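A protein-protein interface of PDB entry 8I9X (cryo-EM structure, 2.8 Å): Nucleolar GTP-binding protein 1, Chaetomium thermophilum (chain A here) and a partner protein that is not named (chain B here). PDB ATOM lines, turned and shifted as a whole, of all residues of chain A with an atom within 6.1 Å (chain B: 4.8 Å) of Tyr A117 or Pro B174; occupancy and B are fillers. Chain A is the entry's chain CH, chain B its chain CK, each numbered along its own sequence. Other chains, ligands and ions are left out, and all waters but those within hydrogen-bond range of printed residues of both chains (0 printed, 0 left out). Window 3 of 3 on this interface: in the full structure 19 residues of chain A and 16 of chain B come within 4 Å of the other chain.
Printed residues of chain B within 4 Å of Tyr A117: Pro B174 (3.8 Å) and Leu B177 (3.98 Å). Pro B174 touches just one residue of chain A: Tyr A117. Printed residues of chain A within 4 Å of Leu B177: Leu A114 (3.7 Å) and Tyr A117 (3.98 Å). Printed residues of chain A within 4 Å of Gly B176: Arg A113 and Leu A114. Of the printed residues of chain B, Arg A113 touches Gly B176. The nearest residue of chain B that does not touch Tyr A117 is Thr B152 (4.02 Å). The nearest printed residue of chain A that does not touch Pro B174 is Arg A113 (7.3 Å). The nearest printed residue of chain A that does not touch Gly B176 is Tyr A117 (5.2 Å).
Among the printed residues, merely in contact across the chains: Arg A113 with Gly B176 (3.9 Å), Leu A114 with Gly B176 (3.6 Å), Leu A114 with Leu B177 (3.7 Å), Tyr A117 with Pro B174 (3.8 Å), Tyr A117 with Leu B177 (3.98 Å) and Gln A119 with Thr B152 (3.4 Å).
NH2 of Arg A42 is in hydrogen-bond range of OE1 of Gln A119, at 3.4 Å. The backbone NH of Gln A119 is in hydrogen-bond range of the side-chain amide oxygen of Gln A123.
Of the 11 printed residues of chain B, 4 touch a printed residue of chain A. Printed residues of chain B that touch a printed residue of chain A: Thr B152, Pro B174, Gly B176 and Leu B177. Hydrophobic or aromatic side chains of chain B within 4 Å of the printed part of chain A: Pro B174 and Leu B177. Hydrophobic or aromatic side chains of chain A that line the printed part of chain B: Leu A114 and Tyr A117. Among the printed residues, no Asp or Glu carboxylate lies within 4 Å of a Lys or Arg side-chain nitrogen of the other chain.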
ATOM      1  N   ARG A  42       9.156  14.900  25.272  1.00  0.00           N
ATOM      2  CA  ARG A  42       8.138  15.912  25.024  1.00  0.00           C
ATOM      3  C   ARG A  42       6.754  15.284  24.956  1.00  0.00           C
ATOM      4  O   ARG A  42       5.791  15.820  25.512  1.00  0.00           O
ATOM      5  CB  ARG A  42       8.446  16.658  23.725  1.00  0.00           C
ATOM      6  CG  ARG A  42       9.641  17.587  23.784  1.00  0.00           C
ATOM      7  CD  ARG A  42      10.000  18.066  22.388  1.00  0.00           C
ATOM      8  NE  ARG A  42      11.280  18.760  22.347  1.00  0.00           N
ATOM      9  CZ  ARG A  42      11.973  18.979  21.237  1.00  0.00           C
ATOM     10  NH1 ARG A  42      11.539  18.565  20.059  1.00  0.00           N
ATOM     11  NH2 ARG A  42      13.131  19.628  21.314  1.00  0.00           N
ATOM     12  N   VAL A 112       1.371  23.156  26.258  1.00  0.00           N
ATOM     13  CA  VAL A 112       1.632  22.178  25.210  1.00  0.00           C
ATOM     14  C   VAL A 112       2.542  22.773  24.143  1.00  0.00           C
ATOM     15  O   VAL A 112       3.466  22.109  23.661  1.00  0.00           O
ATOM     16  CB  VAL A 112       0.313  21.652  24.618  1.00  0.00           C
ATOM     17  CG1 VAL A 112       0.549  21.028  23.255  1.00  0.00           C
ATOM     18  CG2 VAL A 112      -0.304  20.628  25.551  1.00  0.00           C
ATOM     19  N   ARG A 113       2.311  24.032  23.761  1.00  0.00           N
ATOM     20  CA  ARG A 113       3.241  24.675  22.831  1.00  0.00           C
ATOM     21  C   ARG A 113       4.632  24.837  23.453  1.00  0.00           C
ATOM     22  O   ARG A 113       5.663  24.625  22.788  1.00  0.00           O
ATOM     23  CB  ARG A 113       2.685  26.021  22.366  1.00  0.00           C
ATOM     24  CG  ARG A 113       1.459  25.898  21.474  1.00  0.00           C
ATOM     25  CD  ARG A 113       1.064  27.236  20.870  1.00  0.00           C
ATOM     26  NE  ARG A 113       0.655  28.211  21.872  1.00  0.00           N
ATOM     27  CZ  ARG A 113      -0.585  28.342  22.321  1.00  0.00           C
ATOM     28  NH1 ARG A 113      -1.565  27.573  21.877  1.00  0.00           N
ATOM     29  NH2 ARG A 113      -0.849  29.272  23.234  1.00  0.00           N
ATOM     30  N   LEU A 114       4.683  25.209  24.733  1.00  0.00           N
ATOM     31  CA  LEU A 114       5.977  25.343  25.395  1.00  0.00           C
ATOM     32  C   LEU A 114       6.734  24.017  25.415  1.00  0.00           C
ATOM     33  O   LEU A 114       7.946  23.982  25.169  1.00  0.00           O
ATOM     34  CB  LEU A 114       5.789  25.888  26.809  1.00  0.00           C
ATOM     35  CG  LEU A 114       5.376  27.358  26.857  1.00  0.00           C
ATOM     36  CD1 LEU A 114       5.037  27.779  28.273  1.00  0.00           C
ATOM     37  CD2 LEU A 114       6.473  28.234  26.283  1.00  0.00           C
ATOM     38  N   LEU A 115       6.038  22.913  25.695  1.00  0.00           N
ATOM     39  CA  LEU A 115       6.651  21.592  25.632  1.00  0.00           C
ATOM     40  C   LEU A 115       7.034  21.196  24.215  1.00  0.00           C
ATOM     41  O   LEU A 115       8.020  20.475  24.039  1.00  0.00           O
ATOM     42  CB  LEU A 115       5.709  20.544  26.222  1.00  0.00           C
ATOM     43  CG  LEU A 115       5.553  20.576  27.740  1.00  0.00           C
ATOM     44  CD1 LEU A 115       4.205  20.014  28.152  1.00  0.00           C
ATOM     45  CD2 LEU A 115       6.682  19.817  28.406  1.00  0.00           C
ATOM     46  N   LYS A 116       6.262  21.626  23.213  1.00  0.00           N
ATOM     47  CA  LYS A 116       6.687  21.484  21.827  1.00  0.00           C
ATOM     48  C   LYS A 116       8.085  22.036  21.624  1.00  0.00           C
ATOM     49  O   LYS A 116       8.930  21.378  21.008  1.00  0.00           O
ATOM     50  CB  LYS A 116       5.730  22.235  20.903  1.00  0.00           C
ATOM     51  CG  LYS A 116       5.989  22.047  19.420  1.00  0.00           C
ATOM     52  CD  LYS A 116       4.983  22.848  18.613  1.00  0.00           C
ATOM     53  CE  LYS A 116       3.595  22.262  18.690  1.00  0.00           C
ATOM     54  NZ  LYS A 116       3.504  20.946  18.025  1.00  0.00           N
ATOM     55  N   TYR A 117       8.347  23.236  22.137  1.00  0.00           N
ATOM     56  CA  TYR A 117       9.634  23.885  21.896  1.00  0.00           C
ATOM     57  C   TYR A 117      10.603  23.766  23.073  1.00  0.00           C
ATOM     58  O   TYR A 117      11.577  24.521  23.147  1.00  0.00           O
ATOM     59  CB  TYR A 117       9.422  25.345  21.511  1.00  0.00           C
ATOM     60  CG  TYR A 117       8.799  25.497  20.144  1.00  0.00           C
ATOM     61  CD1 TYR A 117       9.553  25.303  18.998  1.00  0.00           C
ATOM     62  CD2 TYR A 117       7.456  25.803  20.000  1.00  0.00           C
ATOM     63  CE1 TYR A 117       8.993  25.433  17.748  1.00  0.00           C
ATOM     64  CE2 TYR A 117       6.885  25.933  18.750  1.00  0.00           C
ATOM     65  CZ  TYR A 117       7.659  25.745  17.627  1.00  0.00           C
ATOM     66  OH  TYR A 117       7.109  25.871  16.373  1.00  0.00           O
ATOM     67  N   ALA A 118      10.363  22.835  23.993  1.00  0.00           N
ATOM     68  CA  ALA A 118      11.317  22.544  25.058  1.00  0.00           C
ATOM     69  C   ALA A 118      12.510  21.772  24.505  1.00  0.00           C
ATOM     70  O   ALA A 118      12.410  21.117  23.466  1.00  0.00           O
ATOM     71  CB  ALA A 118      10.648  21.752  26.180  1.00  0.00           C
ATOM     72  N   GLN A 119      13.645  21.853  25.207  1.00  0.00           N
ATOM     73  CA  GLN A 119      14.906  21.314  24.704  1.00  0.00           C
ATOM     74  C   GLN A 119      15.577  20.340  25.667  1.00  0.00           C
ATOM     75  O   GLN A 119      16.609  19.758  25.324  1.00  0.00           O
ATOM     76  CB  GLN A 119      15.877  22.446  24.367  1.00  0.00           C
ATOM     77  CG  GLN A 119      15.408  23.364  23.260  1.00  0.00           C
ATOM     78  CD  GLN A 119      15.653  22.779  21.888  1.00  0.00           C
ATOM     79  OE1 GLN A 119      14.727  22.612  21.096  1.00  0.00           O
ATOM     80  NE2 GLN A 119      16.908  22.458  21.600  1.00  0.00           N
ATOM     81  N   GLN A 123      13.767  21.018  31.529  1.00  0.00           N
ATOM     82  CA  GLN A 123      12.849  22.059  31.081  1.00  0.00           C
ATOM     83  C   GLN A 123      11.434  21.515  30.934  1.00  0.00           C
ATOM     84  O   GLN A 123      10.458  22.166  31.331  1.00  0.00           O
ATOM     85  CB  GLN A 123      13.342  22.656  29.764  1.00  0.00           C
ATOM     86  CG  GLN A 123      12.548  23.856  29.292  1.00  0.00           C
ATOM     87  CD  GLN A 123      13.082  24.433  28.001  1.00  0.00           C
ATOM     88  OE1 GLN A 123      14.031  23.909  27.420  1.00  0.00           O
ATOM     89  NE2 GLN A 123      12.478  25.523  27.546  1.00  0.00           N
ATOM     90  N   GLU B 130       7.276  31.525  10.751  1.00  0.00           N
ATOM     91  CA  GLU B 130       7.212  30.151  10.259  1.00  0.00           C
ATOM     92  C   GLU B 130       6.523  30.078   8.903  1.00  0.00           C
ATOM     93  O   GLU B 130       7.000  29.386   7.996  1.00  0.00           O
ATOM     94  CB  GLU B 130       6.498  29.251  11.267  1.00  0.00           C
ATOM     95  CG  GLU B 130       7.322  28.912  12.489  1.00  0.00           C
ATOM     96  CD  GLU B 130       7.322  30.016  13.521  1.00  0.00           C
ATOM     97  OE1 GLU B 130       6.587  31.010  13.340  1.00  0.00           O
ATOM     98  OE2 GLU B 130       8.064  29.887  14.513  1.00  0.00           O
ATOM     99  N   ILE B 150      16.075  27.534  15.041  1.00  0.00           N
ATOM    100  CA  ILE B 150      14.949  28.025  15.825  1.00  0.00           C
ATOM    101  C   ILE B 150      15.467  28.592  17.139  1.00  0.00           C
ATOM    102  O   ILE B 150      16.267  27.955  17.834  1.00  0.00           O
ATOM    103  CB  ILE B 150      13.935  26.903  16.073  1.00  0.00           C
ATOM    104  CG1 ILE B 150      13.435  26.336  14.748  1.00  0.00           C
ATOM    105  CG2 ILE B 150      12.776  27.392  16.928  1.00  0.00           C
ATOM    106  CD1 ILE B 150      12.959  27.397  13.818  1.00  0.00           C
ATOM    107  N   VAL B 151      15.007  29.787  17.497  1.00  0.00           N
ATOM    108  CA  VAL B 151      15.263  30.321  18.830  1.00  0.00           C
ATOM    109  C   VAL B 151      14.314  29.632  19.801  1.00  0.00           C
ATOM    110  O   VAL B 151      13.092  29.785  19.705  1.00  0.00           O
ATOM    111  CB  VAL B 151      15.086  31.845  18.869  1.00  0.00           C
ATOM    112  CG1 VAL B 151      15.579  32.397  20.195  1.00  0.00           C
ATOM    113  CG2 VAL B 151      15.827  32.496  17.719  1.00  0.00           C
ATOM    114  N   THR B 152      14.874  28.875  20.742  1.00  0.00           N
ATOM    115  CA  THR B 152      14.087  28.046  21.643  1.00  0.00           C
ATOM    116  C   THR B 152      13.825  28.720  22.982  1.00  0.00           C
ATOM    117  O   THR B 152      13.301  28.077  23.896  1.00  0.00           O
ATOM    118  CB  THR B 152      14.781  26.703  21.866  1.00  0.00           C
ATOM    119  OG1 THR B 152      16.062  26.920  22.469  1.00  0.00           O
ATOM    120  CG2 THR B 152      14.967  25.981  20.545  1.00  0.00           C
ATOM    121  N   ILE B 172      14.122  32.340  13.646  1.00  0.00           N
ATOM    122  CA  ILE B 172      12.683  32.115  13.709  1.00  0.00           C
ATOM    123  C   ILE B 172      12.250  32.084  15.169  1.00  0.00           C
ATOM    124  O   ILE B 172      12.737  31.261  15.953  1.00  0.00           O
ATOM    125  CB  ILE B 172      12.294  30.818  12.983  1.00  0.00           C
ATOM    126  CG1 ILE B 172      12.796  30.848  11.540  1.00  0.00           C
ATOM    127  CG2 ILE B 172      10.794  30.614  13.013  1.00  0.00           C
ATOM    128  CD1 ILE B 172      12.232  31.992  10.728  1.00  0.00           C
ATOM    129  N   ARG B 173      11.341  32.987  15.537  1.00  0.00           N
ATOM    130  CA  ARG B 173      10.832  33.081  16.900  1.00  0.00           C
ATOM    131  C   ARG B 173       9.367  32.675  16.929  1.00  0.00           C
ATOM    132  O   ARG B 173       8.516  33.415  16.415  1.00  0.00           O
ATOM    133  CB  ARG B 173      11.013  34.497  17.437  1.00  0.00           C
ATOM    134  CG  ARG B 173      12.414  35.045  17.220  1.00  0.00           C
ATOM    135  CD  ARG B 173      12.470  36.527  17.499  1.00  0.00           C
ATOM    136  NE  ARG B 173      11.797  37.270  16.443  1.00  0.00           N
ATOM    137  CZ  ARG B 173      11.730  38.591  16.381  1.00  0.00           C
ATOM    138  NH1 ARG B 173      12.303  39.356  17.294  1.00  0.00           N
ATOM    139  NH2 ARG B 173      11.075  39.158  15.373  1.00  0.00           N
ATOM    140  N   PRO B 174       9.025  31.523  17.500  1.00  0.00           N
ATOM    141  CA  PRO B 174       7.660  31.002  17.358  1.00  0.00           C
ATOM    142  C   PRO B 174       6.629  31.713  18.226  1.00  0.00           C
ATOM    143  O   PRO B 174       6.914  32.256  19.301  1.00  0.00           O
ATOM    144  CB  PRO B 174       7.793  29.529  17.762  1.00  0.00           C
ATOM    145  CG  PRO B 174       9.058  29.438  18.515  1.00  0.00           C
ATOM    146  CD  PRO B 174       9.962  30.507  18.008  1.00  0.00           C
ATOM    147  N   MET B 175       5.387  31.660  17.728  1.00  0.00           N
ATOM    148  CA  MET B 175       4.237  32.203  18.443  1.00  0.00           C
ATOM    149  C   MET B 175       4.083  31.582  19.821  1.00  0.00           C
ATOM    150  O   MET B 175       3.732  32.278  20.780  1.00  0.00           O
ATOM    151  CB  MET B 175       2.960  31.967  17.630  1.00  0.00           C
ATOM    152  CG  MET B 175       2.973  32.451  16.177  1.00  0.00           C
ATOM    153  SD  MET B 175       3.587  34.110  15.792  1.00  0.00           S
ATOM    154  CE  MET B 175       3.083  35.071  17.223  1.00  0.00           C
ATOM    155  N   GLY B 176       4.332  30.277  19.939  1.00  0.00           N
ATOM    156  CA  GLY B 176       4.223  29.621  21.225  1.00  0.00           C
ATOM    157  C   GLY B 176       5.213  30.123  22.250  1.00  0.00           C
ATOM    158  O   GLY B 176       4.985  29.953  23.450  1.00  0.00           O
ATOM    159  N   LEU B 177       6.309  30.735  21.804  1.00  0.00           N
ATOM    160  CA  LEU B 177       7.336  31.241  22.698  1.00  0.00           C
ATOM    161  C   LEU B 177       7.249  32.750  22.903  1.00  0.00           C
ATOM    162  O   LEU B 177       7.832  33.269  23.860  1.00  0.00           O
ATOM    163  CB  LEU B 177       8.723  30.860  22.180  1.00  0.00           C
ATOM    164  CG  LEU B 177       9.167  29.414  22.413  1.00  0.00           C
ATOM    165  CD1 LEU B 177      10.521  29.160  21.779  1.00  0.00           C
ATOM    166  CD2 LEU B 177       9.202  29.091  23.894  1.00  0.00           C
ATOM    167  N   ARG B 178       6.537  33.467  22.036  1.00  0.00           N
ATOM    168  CA  ARG B 178       6.387  34.913  22.177  1.00  0.00           C
ATOM    169  C   ARG B 178       5.554  35.249  23.410  1.00  0.00           C
ATOM    170  O   ARG B 178       4.576  34.559  23.711  1.00  0.00           O
ATOM    171  CB  ARG B 178       5.751  35.536  20.934  1.00  0.00           C
ATOM    172  CG  ARG B 178       6.482  35.223  19.652  1.00  0.00           C
ATOM    173  CD  ARG B 178       6.165  36.219  18.562  1.00  0.00           C
ATOM    174  NE  ARG B 178       7.142  36.140  17.486  1.00  0.00           N
ATOM    175  CZ  ARG B 178       6.851  36.239  16.198  1.00  0.00           C
ATOM    176  NH1 ARG B 178       5.615  36.451  15.782  1.00  0.00           N
ATOM    177  NH2 ARG B 178       7.827  36.131  15.305  1.00  0.00           N
